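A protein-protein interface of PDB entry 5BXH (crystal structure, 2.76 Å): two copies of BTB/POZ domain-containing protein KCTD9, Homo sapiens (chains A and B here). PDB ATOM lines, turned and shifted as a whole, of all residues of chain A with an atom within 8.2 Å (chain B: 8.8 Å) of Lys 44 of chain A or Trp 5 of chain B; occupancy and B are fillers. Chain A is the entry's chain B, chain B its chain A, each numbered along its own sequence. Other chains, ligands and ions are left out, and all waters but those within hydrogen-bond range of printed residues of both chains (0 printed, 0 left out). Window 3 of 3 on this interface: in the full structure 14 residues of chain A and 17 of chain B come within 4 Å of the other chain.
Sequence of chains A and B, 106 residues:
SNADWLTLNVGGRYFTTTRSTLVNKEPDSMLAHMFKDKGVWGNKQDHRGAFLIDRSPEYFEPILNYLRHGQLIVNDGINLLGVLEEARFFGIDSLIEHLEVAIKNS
Positions printed for both chains: 7, 49 and 51.
Of the 13 pairs that touch across the chains among the printed residues, none has its exchanged pair printed and touching as well.
The backbone NH of Leu 6 of chain B sits at hydrogen-bond distance from the backbone carbonyl oxygen of Thr 17 of chain B.
The backbone NH (N) of Leu 8 of chain B is in hydrogen-bond range of the backbone carbonyl oxygen (O) of Phe 15 of chain B (2.9 Å).
The side-chain hydroxyl of Thr 21 of chain B sits at hydrogen-bond distance from the side-chain hydroxyl of Thr 18 of chain B (2.6 Å).
The side-chain amide oxygen (OD1) of Asn 9 of chain A lies within hydrogen-bond range of the backbone NH (N) of Gly 12 of chain A, at 3.1 Å.
O of Ile 53 of chain A sits at hydrogen-bond distance from N of Gly 11 of chain A (3.0 Å).
Of the 18 printed residues of chain B, 7 touch a printed residue of chain A.
Printed residues of chain B that touch a printed residue of chain A: Trp 5, Phe 15, Thr 16, Thr 17, Thr 18, Thr 21 and Arg 68.
Hydrophobic or aromatic side chains of chain B within 4 Å of the printed part of chain A: Trp 5 and Phe 15.
Among the printed residues, Asp or Glu carboxylates within 4 Å of a Lys or Arg side-chain nitrogen of the other chain: Asp 54 of chain A with Arg 68 of chain B.
Phe 15 of chain B touches Gly 11 of chain A.
Thr 16 of chain B touches Gly 12 of chain A (OG1 to CA, 3.5 Å).
NE1 of Trp 5 of chain B touches CG of Lys 44 of chain A (3.4 Å).
CB of Leu 52 of chain A touches CZ2 of Trp 5 of chain B (3.5 Å).
Thr 16 of chain B touches Leu 52 of chain A (CG2 to CD2, 3.8 Å).
Asp 54 of chain A touches Trp 5 of chain B (N to CH2, 3.8 Å).
Thr 16 of chain B touches Asp 54 of chain A (O to OD1, 3.9 Å).
O of Gly 11 of chain A is in hydrogen-bond range of N of Thr 16 of chain B (2.9 Å).
The side-chain hydroxyl (OG1) of Thr 17 of chain B sits at hydrogen-bond distance from the side-chain carboxylate (OD1) of Asp 54 of chain A.
OD2 of Asp 54 of chain A sits at hydrogen-bond distance from OG1 of Thr 18 of chain B, 3.1 Å away.
The side-chain hydroxyl (OG1) of Thr 21 of chain B lies within hydrogen-bond range of the side-chain carboxylate (OD2) of Asp 54 of chain A (2.7 Å).
OD1 of Asp 54 of chain A lies within salt-bridge range of NH1 of Arg 68 of chain B (2.5 Å).
The backbone carbonyl oxygen (O) of Arg 55 of chain A sits close to the guanidinium group (NH1) of Arg 68 of chain B (3.3 Å).
Lys 44 of chain A touches just one residue of chain B: Trp 5.
Printed residues of chain A within 4 Å of Trp 5 of chain B: Lys 44, Leu 52 and Asp 54.
Of the printed residues of chain A, Arg 68 of chain B touches Asp 54 and Arg 55.
Printed residues of chain B within 4 Å of Gly 12 of chain A: Thr 16.
Phe 51 of chain B touches none of the printed residues of chain A.
Ala 3 of chain B touches none of the printed residues of chain A.
The nearest residue of chain B that does not touch Lys 44 of chain A is Ala 3 of chain B (5.3 Å).
The nearest printed residue of chain A that does not touch Trp 5 of chain B is Ile 53 of chain A (4.01 Å).
The nearest printed residue of chain A that does not touch Phe 15 of chain B is Gly 12 of chain A (4.4 Å).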
ATOM      1  N   THR A   7       8.551 -24.692 -27.233  1.00  0.00           N
ATOM      2  CA  THR A   7       7.901 -25.171 -26.022  1.00  0.00           C
ATOM      3  C   THR A   7       6.448 -25.518 -26.332  1.00  0.00           C
ATOM      4  O   THR A   7       5.750 -24.753 -26.994  1.00  0.00           O
ATOM      5  CB  THR A   7       7.959 -24.125 -24.893  1.00  0.00           C
ATOM      6  OG1 THR A   7       9.275 -23.561 -24.829  1.00  0.00           O
ATOM      7  CG2 THR A   7       7.615 -24.760 -23.554  1.00  0.00           C
ATOM      8  N   ASN A   9       2.741 -26.604 -24.722  1.00  0.00           N
ATOM      9  CA  ASN A   9       1.875 -26.698 -23.553  1.00  0.00           C
ATOM     10  C   ASN A   9       0.806 -27.759 -23.779  1.00  0.00           C
ATOM     11  O   ASN A   9      -0.251 -27.474 -24.338  1.00  0.00           O
ATOM     12  CB  ASN A   9       1.230 -25.342 -23.249  1.00  0.00           C
ATOM     13  CG  ASN A   9       0.527 -25.310 -21.901  1.00  0.00           C
ATOM     14  OD1 ASN A   9       0.124 -26.343 -21.367  1.00  0.00           O
ATOM     15  ND2 ASN A   9       0.372 -24.111 -21.349  1.00  0.00           N
ATOM     16  N   VAL A  10       1.086 -28.985 -23.349  1.00  0.00           N
ATOM     17  CA  VAL A  10       0.138 -30.078 -23.516  1.00  0.00           C
ATOM     18  C   VAL A  10      -0.670 -30.292 -22.240  1.00  0.00           C
ATOM     19  O   VAL A  10      -0.145 -30.766 -21.230  1.00  0.00           O
ATOM     20  CB  VAL A  10       0.846 -31.390 -23.900  1.00  0.00           C
ATOM     21  CG1 VAL A  10      -0.172 -32.493 -24.135  1.00  0.00           C
ATOM     22  CG2 VAL A  10       1.706 -31.185 -25.136  1.00  0.00           C
ATOM     23  N   GLY A  11      -1.943 -29.913 -22.288  1.00  0.00           N
ATOM     24  CA  GLY A  11      -2.863 -30.135 -21.187  1.00  0.00           C
ATOM     25  C   GLY A  11      -2.539 -29.414 -19.891  1.00  0.00           C
ATOM     26  O   GLY A  11      -3.183 -29.653 -18.871  1.00  0.00           O
ATOM     27  N   GLY A  12      -1.548 -28.528 -19.926  1.00  0.00           N
ATOM     28  CA  GLY A  12      -1.120 -27.815 -18.736  1.00  0.00           C
ATOM     29  C   GLY A  12       0.316 -28.133 -18.365  1.00  0.00           C
ATOM     30  O   GLY A  12       0.893 -27.510 -17.473  1.00  0.00           O
ATOM     31  N   MET A  34       2.052 -28.577 -38.053  1.00  0.00           N
ATOM     32  CA  MET A  34       1.749 -27.505 -37.114  1.00  0.00           C
ATOM     33  C   MET A  34       2.889 -26.497 -37.000  1.00  0.00           C
ATOM     34  O   MET A  34       2.656 -25.308 -36.786  1.00  0.00           O
ATOM     35  CB  MET A  34       1.435 -28.076 -35.732  1.00  0.00           C
ATOM     36  CG  MET A  34       0.063 -28.700 -35.612  1.00  0.00           C
ATOM     37  SD  MET A  34      -0.287 -29.214 -33.923  1.00  0.00           S
ATOM     38  CE  MET A  34      -0.156 -27.646 -33.066  1.00  0.00           C
ATOM     39  N   PHE A  35       4.120 -26.977 -37.144  1.00  0.00           N
ATOM     40  CA  PHE A  35       5.291 -26.140 -36.905  1.00  0.00           C
ATOM     41  C   PHE A  35       6.188 -26.013 -38.135  1.00  0.00           C
ATOM     42  O   PHE A  35       7.229 -26.661 -38.221  1.00  0.00           O
ATOM     43  CB  PHE A  35       6.103 -26.697 -35.730  1.00  0.00           C
ATOM     44  CG  PHE A  35       5.276 -27.011 -34.515  1.00  0.00           C
ATOM     45  CD1 PHE A  35       4.935 -26.015 -33.615  1.00  0.00           C
ATOM     46  CD2 PHE A  35       4.842 -28.304 -34.270  1.00  0.00           C
ATOM     47  CE1 PHE A  35       4.173 -26.302 -32.497  1.00  0.00           C
ATOM     48  CE2 PHE A  35       4.081 -28.597 -33.157  1.00  0.00           C
ATOM     49  CZ  PHE A  35       3.746 -27.595 -32.268  1.00  0.00           C
ATOM     50  N   ASN A  43      -3.056 -20.178 -35.404  1.00  0.00           N
ATOM     51  CA  ASN A  43      -2.549 -20.834 -34.204  1.00  0.00           C
ATOM     52  C   ASN A  43      -2.789 -20.015 -32.942  1.00  0.00           C
ATOM     53  O   ASN A  43      -3.508 -19.015 -32.967  1.00  0.00           O
ATOM     54  CB  ASN A  43      -1.057 -21.134 -34.350  1.00  0.00           C
ATOM     55  CG  ASN A  43      -0.795 -22.534 -34.863  1.00  0.00           C
ATOM     56  OD1 ASN A  43      -1.483 -23.483 -34.486  1.00  0.00           O
ATOM     57  ND2 ASN A  43       0.204 -22.672 -35.728  1.00  0.00           N
ATOM     58  N   LYS A  44      -2.180 -20.444 -31.840  1.00  0.00           N
ATOM     59  CA  LYS A  44      -2.409 -19.815 -30.543  1.00  0.00           C
ATOM     60  C   LYS A  44      -1.142 -19.774 -29.682  1.00  0.00           C
ATOM     61  O   LYS A  44      -0.305 -20.676 -29.738  1.00  0.00           O
ATOM     62  CB  LYS A  44      -3.531 -20.549 -29.800  1.00  0.00           C
ATOM     63  CG  LYS A  44      -3.929 -19.925 -28.470  1.00  0.00           C
ATOM     64  CD  LYS A  44      -4.352 -18.475 -28.637  1.00  0.00           C
ATOM     65  CE  LYS A  44      -4.726 -17.853 -27.301  1.00  0.00           C
ATOM     66  NZ  LYS A  44      -3.606 -17.908 -26.321  1.00  0.00           N
ATOM     67  N   GLN A  45      -1.016 -18.712 -28.891  1.00  0.00           N
ATOM     68  CA  GLN A  45       0.122 -18.508 -28.000  1.00  0.00           C
ATOM     69  C   GLN A  45      -0.351 -18.366 -26.548  1.00  0.00           C
ATOM     70  O   GLN A  45      -1.300 -17.632 -26.274  1.00  0.00           O
ATOM     71  CB  GLN A  45       0.909 -17.266 -28.432  1.00  0.00           C
ATOM     72  CG  GLN A  45       0.026 -16.040 -28.685  1.00  0.00           C
ATOM     73  CD  GLN A  45       0.797 -14.831 -29.188  1.00  0.00           C
ATOM     74  OE1 GLN A  45       1.954 -14.939 -29.594  1.00  0.00           O
ATOM     75  NE2 GLN A  45       0.153 -13.667 -29.162  1.00  0.00           N
ATOM     76  N   ASP A  46       0.296 -19.067 -25.618  1.00  0.00           N
ATOM     77  CA  ASP A  46      -0.073 -18.958 -24.206  1.00  0.00           C
ATOM     78  C   ASP A  46       0.706 -17.825 -23.528  1.00  0.00           C
ATOM     79  O   ASP A  46       1.330 -17.008 -24.203  1.00  0.00           O
ATOM     80  CB  ASP A  46       0.160 -20.287 -23.476  1.00  0.00           C
ATOM     81  CG  ASP A  46       1.607 -20.487 -23.064  1.00  0.00           C
ATOM     82  OD1 ASP A  46       2.505 -20.236 -23.892  1.00  0.00           O
ATOM     83  OD2 ASP A  46       1.839 -20.878 -21.904  1.00  0.00           O
ATOM     84  N   HIS A  47       0.664 -17.777 -22.198  1.00  0.00           N
ATOM     85  CA  HIS A  47       1.313 -16.703 -21.449  1.00  0.00           C
ATOM     86  C   HIS A  47       2.828 -16.895 -21.347  1.00  0.00           C
ATOM     87  O   HIS A  47       3.543 -15.993 -20.911  1.00  0.00           O
ATOM     88  CB  HIS A  47       0.711 -16.589 -20.044  1.00  0.00           C
ATOM     89  CG  HIS A  47       1.125 -17.692 -19.121  1.00  0.00           C
ATOM     90  ND1 HIS A  47       0.499 -18.917 -19.097  1.00  0.00           N
ATOM     91  CD2 HIS A  47       2.115 -17.756 -18.196  1.00  0.00           C
ATOM     92  CE1 HIS A  47       1.079 -19.690 -18.196  1.00  0.00           C
ATOM     93  NE2 HIS A  47       2.063 -19.008 -17.635  1.00  0.00           N
ATOM     94  N   GLY A  49       4.556 -18.209 -24.133  1.00  0.00           N
ATOM     95  CA  GLY A  49       5.002 -18.328 -25.511  1.00  0.00           C
ATOM     96  C   GLY A  49       4.781 -19.697 -26.130  1.00  0.00           C
ATOM     97  O   GLY A  49       4.780 -19.838 -27.353  1.00  0.00           O
ATOM     98  N   ALA A  50       4.592 -20.703 -25.280  1.00  0.00           N
ATOM     99  CA  ALA A  50       4.425 -22.083 -25.730  1.00  0.00           C
ATOM    100  C   ALA A  50       3.164 -22.244 -26.569  1.00  0.00           C
ATOM    101  O   ALA A  50       2.245 -21.431 -26.492  1.00  0.00           O
ATOM    102  CB  ALA A  50       4.390 -23.029 -24.538  1.00  0.00           C
ATOM    103  N   PHE A  51       3.123 -23.299 -27.374  1.00  0.00           N
ATOM    104  CA  PHE A  51       1.963 -23.552 -28.212  1.00  0.00           C
ATOM    105  C   PHE A  51       1.032 -24.549 -27.527  1.00  0.00           C
ATOM    106  O   PHE A  51       1.464 -25.599 -27.052  1.00  0.00           O
ATOM    107  CB  PHE A  51       2.399 -24.042 -29.597  1.00  0.00           C
ATOM    108  CG  PHE A  51       3.249 -23.046 -30.349  1.00  0.00           C
ATOM    109  CD1 PHE A  51       2.667 -22.002 -31.054  1.00  0.00           C
ATOM    110  CD2 PHE A  51       4.633 -23.147 -30.338  1.00  0.00           C
ATOM    111  CE1 PHE A  51       3.450 -21.081 -31.739  1.00  0.00           C
ATOM    112  CE2 PHE A  51       5.420 -22.230 -31.021  1.00  0.00           C
ATOM    113  CZ  PHE A  51       4.828 -21.197 -31.721  1.00  0.00           C
ATOM    114  N   LEU A  52      -0.248 -24.196 -27.473  1.00  0.00           N
ATOM    115  CA  LEU A  52      -1.240 -24.942 -26.705  1.00  0.00           C
ATOM    116  C   LEU A  52      -1.762 -26.180 -27.431  1.00  0.00           C
ATOM    117  O   LEU A  52      -2.159 -26.111 -28.594  1.00  0.00           O
ATOM    118  CB  LEU A  52      -2.407 -24.022 -26.345  1.00  0.00           C
ATOM    119  CG  LEU A  52      -2.053 -22.882 -25.389  1.00  0.00           C
ATOM    120  CD1 LEU A  52      -3.111 -21.798 -25.422  1.00  0.00           C
ATOM    121  CD2 LEU A  52      -1.881 -23.422 -23.978  1.00  0.00           C
ATOM    122  N   ILE A  53      -1.752 -27.309 -26.729  1.00  0.00           N
ATOM    123  CA  ILE A  53      -2.297 -28.560 -27.244  1.00  0.00           C
ATOM    124  C   ILE A  53      -3.238 -29.177 -26.210  1.00  0.00           C
ATOM    125  O   ILE A  53      -2.850 -29.406 -25.063  1.00  0.00           O
ATOM    126  CB  ILE A  53      -1.185 -29.569 -27.595  1.00  0.00           C
ATOM    127  CG1 ILE A  53      -0.279 -29.013 -28.696  1.00  0.00           C
ATOM    128  CG2 ILE A  53      -1.786 -30.899 -28.022  1.00  0.00           C
ATOM    129  CD1 ILE A  53       0.944 -29.873 -28.976  1.00  0.00           C
ATOM    130  N   ASP A  54      -4.473 -29.443 -26.622  1.00  0.00           N
ATOM    131  CA  ASP A  54      -5.506 -29.942 -25.717  1.00  0.00           C
ATOM    132  C   ASP A  54      -5.557 -31.470 -25.698  1.00  0.00           C
ATOM    133  O   ASP A  54      -6.543 -32.068 -26.129  1.00  0.00           O
ATOM    134  CB  ASP A  54      -6.870 -29.365 -26.117  1.00  0.00           C
ATOM    135  CG  ASP A  54      -7.961 -29.666 -25.104  1.00  0.00           C
ATOM    136  OD1 ASP A  54      -7.637 -30.108 -23.981  1.00  0.00           O
ATOM    137  OD2 ASP A  54      -9.148 -29.449 -25.431  1.00  0.00           O
ATOM    138  N   ARG A  55      -4.488 -32.095 -25.205  1.00  0.00           N
ATOM    139  CA  ARG A  55      -4.427 -33.551 -25.066  1.00  0.00           C
ATOM    140  C   ARG A  55      -3.828 -33.942 -23.716  1.00  0.00           C
ATOM    141  O   ARG A  55      -3.530 -33.082 -22.888  1.00  0.00           O
ATOM    142  CB  ARG A  55      -3.599 -34.179 -26.194  1.00  0.00           C
ATOM    143  CG  ARG A  55      -4.027 -33.802 -27.607  1.00  0.00           C
ATOM    144  CD  ARG A  55      -5.415 -34.319 -27.946  1.00  0.00           C
ATOM    145  NE  ARG A  55      -5.485 -35.776 -27.953  1.00  0.00           N
ATOM    146  CZ  ARG A  55      -6.597 -36.464 -28.184  1.00  0.00           C
ATOM    147  NH1 ARG A  55      -7.731 -35.822 -28.427  1.00  0.00           N
ATOM    148  NH2 ARG A  55      -6.578 -37.789 -28.173  1.00  0.00           N
ATOM    149  N   ASN B   2     -12.030 -25.320 -29.132  1.00  0.00           N
ATOM    150  CA  ASN B   2     -11.285 -25.123 -30.370  1.00  0.00           C
ATOM    151  C   ASN B   2     -10.497 -23.816 -30.366  1.00  0.00           C
ATOM    152  O   ASN B   2      -9.292 -23.807 -30.618  1.00  0.00           O
ATOM    153  CB  ASN B   2     -12.233 -25.154 -31.574  1.00  0.00           C
ATOM    154  CG  ASN B   2     -11.511 -24.958 -32.897  1.00  0.00           C
ATOM    155  OD1 ASN B   2     -10.343 -25.323 -33.044  1.00  0.00           O
ATOM    156  ND2 ASN B   2     -12.205 -24.376 -33.869  1.00  0.00           N
ATOM    157  N   ALA B   3     -11.183 -22.716 -30.071  1.00  0.00           N
ATOM    158  CA  ALA B   3     -10.574 -21.394 -30.151  1.00  0.00           C
ATOM    159  C   ALA B   3     -10.391 -20.743 -28.781  1.00  0.00           C
ATOM    160  O   ALA B   3      -9.452 -19.974 -28.577  1.00  0.00           O
ATOM    161  CB  ALA B   3     -11.407 -20.490 -31.054  1.00  0.00           C
ATOM    162  N   ASP B   4     -11.285 -21.052 -27.845  1.00  0.00           N
ATOM    163  CA  ASP B   4     -11.268 -20.403 -26.536  1.00  0.00           C
ATOM    164  C   ASP B   4     -10.567 -21.264 -25.486  1.00  0.00           C
ATOM    165  O   ASP B   4     -11.051 -22.334 -25.118  1.00  0.00           O
ATOM    166  CB  ASP B   4     -12.693 -20.079 -26.085  1.00  0.00           C
ATOM    167  CG  ASP B   4     -12.746 -18.927 -25.099  1.00  0.00           C
ATOM    168  OD1 ASP B   4     -11.733 -18.680 -24.412  1.00  0.00           O
ATOM    169  OD2 ASP B   4     -13.803 -18.266 -25.015  1.00  0.00           O
ATOM    170  N   TRP B   5      -9.431 -20.780 -24.999  1.00  0.00           N
ATOM    171  CA  TRP B   5      -8.617 -21.545 -24.060  1.00  0.00           C
ATOM    172  C   TRP B   5      -8.900 -21.175 -22.608  1.00  0.00           C
ATOM    173  O   TRP B   5      -9.027 -20.000 -22.264  1.00  0.00           O
ATOM    174  CB  TRP B   5      -7.131 -21.352 -24.371  1.00  0.00           C
ATOM    175  CG  TRP B   5      -6.712 -21.990 -25.663  1.00  0.00           C
ATOM    176  CD1 TRP B   5      -6.648 -21.395 -26.891  1.00  0.00           C
ATOM    177  CD2 TRP B   5      -6.310 -23.352 -25.855  1.00  0.00           C
ATOM    178  NE1 TRP B   5      -6.226 -22.303 -27.834  1.00  0.00           N
ATOM    179  CE2 TRP B   5      -6.013 -23.511 -27.224  1.00  0.00           C
ATOM    180  CE3 TRP B   5      -6.169 -24.452 -25.003  1.00  0.00           C
ATOM    181  CZ2 TRP B   5      -5.585 -24.725 -27.760  1.00  0.00           C
ATOM    182  CZ3 TRP B   5      -5.745 -25.655 -25.536  1.00  0.00           C
ATOM    183  CH2 TRP B   5      -5.457 -25.782 -26.902  1.00  0.00           C
ATOM    184  N   LEU B   6      -8.997 -22.196 -21.763  1.00  0.00           N
ATOM    185  CA  LEU B   6      -9.233 -22.012 -20.338  1.00  0.00           C
ATOM    186  C   LEU B   6      -8.221 -22.789 -19.503  1.00  0.00           C
ATOM    187  O   LEU B   6      -7.761 -23.866 -19.899  1.00  0.00           O
ATOM    188  CB  LEU B   6     -10.650 -22.450 -19.966  1.00  0.00           C
ATOM    189  CG  LEU B   6     -11.818 -21.742 -20.649  1.00  0.00           C
ATOM    190  CD1 LEU B   6     -13.121 -22.433 -20.289  1.00  0.00           C
ATOM    191  CD2 LEU B   6     -11.862 -20.272 -20.260  1.00  0.00           C
ATOM    192  N   THR B   7      -7.885 -22.237 -18.345  1.00  0.00           N
ATOM    193  CA  THR B   7      -7.024 -22.919 -17.391  1.00  0.00           C
ATOM    194  C   THR B   7      -7.804 -23.221 -16.117  1.00  0.00           C
ATOM    195  O   THR B   7      -8.459 -22.343 -15.557  1.00  0.00           O
ATOM    196  CB  THR B   7      -5.783 -22.084 -17.049  1.00  0.00           C
ATOM    197  OG1 THR B   7      -5.226 -21.536 -18.250  1.00  0.00           O
ATOM    198  CG2 THR B   7      -4.744 -22.943 -16.352  1.00  0.00           C
ATOM    199  N   LEU B   8      -7.743 -24.470 -15.671  1.00  0.00           N
ATOM    200  CA  LEU B   8      -8.431 -24.886 -14.460  1.00  0.00           C
ATOM    201  C   LEU B   8      -7.435 -25.199 -13.352  1.00  0.00           C
ATOM    202  O   LEU B   8      -6.499 -25.976 -13.549  1.00  0.00           O
ATOM    203  CB  LEU B   8      -9.309 -26.108 -14.732  1.00  0.00           C
ATOM    204  CG  LEU B   8     -10.312 -26.024 -15.885  1.00  0.00           C
ATOM    205  CD1 LEU B   8     -11.157 -27.288 -15.939  1.00  0.00           C
ATOM    206  CD2 LEU B   8     -11.189 -24.788 -15.761  1.00  0.00           C
ATOM    207  N   PHE B  15      -4.544 -27.441 -15.116  1.00  0.00           N
ATOM    208  CA  PHE B  15      -4.847 -28.106 -16.376  1.00  0.00           C
ATOM    209  C   PHE B  15      -5.206 -27.053 -17.413  1.00  0.00           C
ATOM    210  O   PHE B  15      -5.817 -26.045 -17.085  1.00  0.00           O
ATOM    211  CB  PHE B  15      -5.996 -29.102 -16.211  1.00  0.00           C
ATOM    212  CG  PHE B  15      -5.687 -30.242 -15.284  1.00  0.00           C
ATOM    213  CD1 PHE B  15      -5.770 -30.078 -13.910  1.00  0.00           C
ATOM    214  CD2 PHE B  15      -5.327 -31.482 -15.785  1.00  0.00           C
ATOM    215  CE1 PHE B  15      -5.491 -31.125 -13.054  1.00  0.00           C
ATOM    216  CE2 PHE B  15      -5.048 -32.535 -14.934  1.00  0.00           C
ATOM    217  CZ  PHE B  15      -5.131 -32.356 -13.566  1.00  0.00           C
ATOM    218  N   THR B  16      -4.823 -27.275 -18.662  1.00  0.00           N
ATOM    219  CA  THR B  16      -5.195 -26.341 -19.715  1.00  0.00           C
ATOM    220  C   THR B  16      -6.021 -27.048 -20.780  1.00  0.00           C
ATOM    221  O   THR B  16      -5.634 -28.107 -21.276  1.00  0.00           O
ATOM    222  CB  THR B  16      -3.961 -25.687 -20.358  1.00  0.00           C
ATOM    223  OG1 THR B  16      -3.194 -25.016 -19.350  1.00  0.00           O
ATOM    224  CG2 THR B  16      -4.386 -24.676 -21.409  1.00  0.00           C
ATOM    225  N   THR B  17      -7.167 -26.467 -21.120  1.00  0.00           N
ATOM    226  CA  THR B  17      -8.044 -27.064 -22.124  1.00  0.00           C
ATOM    227  C   THR B  17      -8.861 -26.007 -22.864  1.00  0.00           C
ATOM    228  O   THR B  17      -8.535 -24.825 -22.824  1.00  0.00           O
ATOM    229  CB  THR B  17      -8.999 -28.092 -21.491  1.00  0.00           C
ATOM    230  OG1 THR B  17      -9.806 -28.688 -22.513  1.00  0.00           O
ATOM    231  CG2 THR B  17      -9.896 -27.428 -20.453  1.00  0.00           C
ATOM    232  N   THR B  18      -9.911 -26.441 -23.553  1.00  0.00           N
ATOM    233  CA  THR B  18     -10.792 -25.514 -24.260  1.00  0.00           C
ATOM    234  C   THR B  18     -12.216 -25.587 -23.727  1.00  0.00           C
ATOM    235  O   THR B  18     -12.671 -26.643 -23.285  1.00  0.00           O
ATOM    236  CB  THR B  18     -10.817 -25.791 -25.774  1.00  0.00           C
ATOM    237  OG1 THR B  18     -11.175 -27.158 -26.007  1.00  0.00           O
ATOM    238  CG2 THR B  18      -9.456 -25.517 -26.390  1.00  0.00           C
ATOM    239  N   ARG B  19     -12.910 -24.454 -23.773  1.00  0.00           N
ATOM    240  CA  ARG B  19     -14.305 -24.374 -23.354  1.00  0.00           C
ATOM    241  C   ARG B  19     -15.149 -25.404 -24.097  1.00  0.00           C
ATOM    242  O   ARG B  19     -16.048 -26.026 -23.521  1.00  0.00           O
ATOM    243  CB  ARG B  19     -14.854 -22.968 -23.595  1.00  0.00           C
ATOM    244  CG  ARG B  19     -16.261 -22.758 -23.083  1.00  0.00           C
ATOM    245  CD  ARG B  19     -16.792 -21.394 -23.483  1.00  0.00           C
ATOM    246  NE  ARG B  19     -15.871 -20.321 -23.119  1.00  0.00           N
ATOM    247  CZ  ARG B  19     -15.768 -19.812 -21.896  1.00  0.00           C
ATOM    248  NH1 ARG B  19     -16.525 -20.283 -20.915  1.00  0.00           N
ATOM    249  NH2 ARG B  19     -14.906 -18.835 -21.653  1.00  0.00           N
ATOM    250  N   SER B  20     -14.836 -25.575 -25.378  1.00  0.00           N
ATOM    251  CA  SER B  20     -15.485 -26.563 -26.232  1.00  0.00           C
ATOM    252  C   SER B  20     -15.447 -27.959 -25.620  1.00  0.00           C
ATOM    253  O   SER B  20     -16.439 -28.684 -25.641  1.00  0.00           O
ATOM    254  CB  SER B  20     -14.818 -26.583 -27.609  1.00  0.00           C
ATOM    255  OG  SER B  20     -15.282 -27.674 -28.384  1.00  0.00           O
ATOM    256  N   THR B  21     -14.297 -28.325 -25.070  1.00  0.00           N
ATOM    257  CA  THR B  21     -14.125 -29.639 -24.466  1.00  0.00           C
ATOM    258  C   THR B  21     -14.941 -29.768 -23.180  1.00  0.00           C
ATOM    259  O   THR B  21     -15.437 -30.846 -22.854  1.00  0.00           O
ATOM    260  CB  THR B  21     -12.641 -29.925 -24.167  1.00  0.00           C
ATOM    261  OG1 THR B  21     -11.845 -29.545 -25.297  1.00  0.00           O
ATOM    262  CG2 THR B  21     -12.425 -31.401 -23.873  1.00  0.00           C
ATOM    263  N   LEU B  22     -15.091 -28.660 -22.462  1.00  0.00           N
ATOM    264  CA  LEU B  22     -15.787 -28.667 -21.179  1.00  0.00           C
ATOM    265  C   LEU B  22     -17.314 -28.631 -21.317  1.00  0.00           C
ATOM    266  O   LEU B  22     -18.025 -29.102 -20.427  1.00  0.00           O
ATOM    267  CB  LEU B  22     -15.317 -27.488 -20.319  1.00  0.00           C
ATOM    268  CG  LEU B  22     -13.861 -27.524 -19.837  1.00  0.00           C
ATOM    269  CD1 LEU B  22     -13.465 -26.207 -19.184  1.00  0.00           C
ATOM    270  CD2 LEU B  22     -13.630 -28.683 -18.877  1.00  0.00           C
ATOM    271  N   GLY B  49      -5.424 -16.508 -12.970  1.00  0.00           N
ATOM    272  CA  GLY B  49      -6.682 -16.362 -13.678  1.00  0.00           C
ATOM    273  C   GLY B  49      -7.388 -17.685 -13.904  1.00  0.00           C
ATOM    274  O   GLY B  49      -8.443 -17.738 -14.537  1.00  0.00           O
ATOM    275  N   PHE B  51      -9.629 -20.917 -13.158  1.00  0.00           N
ATOM    276  CA  PHE B  51     -10.844 -21.172 -12.397  1.00  0.00           C
ATOM    277  C   PHE B  51     -10.588 -22.243 -11.339  1.00  0.00           C
ATOM    278  O   PHE B  51     -10.107 -23.332 -11.649  1.00  0.00           O
ATOM    279  CB  PHE B  51     -11.984 -21.587 -13.330  1.00  0.00           C
ATOM    280  CG  PHE B  51     -12.403 -20.507 -14.292  1.00  0.00           C
ATOM    281  CD1 PHE B  51     -13.389 -19.597 -13.946  1.00  0.00           C
ATOM    282  CD2 PHE B  51     -11.806 -20.397 -15.539  1.00  0.00           C
ATOM    283  CE1 PHE B  51     -13.773 -18.601 -14.827  1.00  0.00           C
ATOM    284  CE2 PHE B  51     -12.187 -19.401 -16.425  1.00  0.00           C
ATOM    285  CZ  PHE B  51     -13.172 -18.503 -16.068  1.00  0.00           C
ATOM    286  N   ARG B  68     -12.147 -35.206 -23.593  1.00  0.00           N
ATOM    287  CA  ARG B  68     -11.406 -34.936 -24.820  1.00  0.00           C
ATOM    288  C   ARG B  68     -11.716 -35.930 -25.943  1.00  0.00           C
ATOM    289  O   ARG B  68     -11.922 -35.526 -27.088  1.00  0.00           O
ATOM    290  CB  ARG B  68      -9.899 -34.927 -24.537  1.00  0.00           C
ATOM    291  CG  ARG B  68      -9.413 -33.724 -23.728  1.00  0.00           C
ATOM    292  CD  ARG B  68      -7.897 -33.588 -23.790  1.00  0.00           C
ATOM    293  NE  ARG B  68      -7.241 -33.800 -22.500  1.00  0.00           N
ATOM    294  CZ  ARG B  68      -6.552 -32.868 -21.846  1.00  0.00           C
ATOM    295  NH1 ARG B  68      -6.419 -31.651 -22.357  1.00  0.00           N
ATOM    296  NH2 ARG B  68      -5.987 -33.156 -20.681  1.00  0.00           N
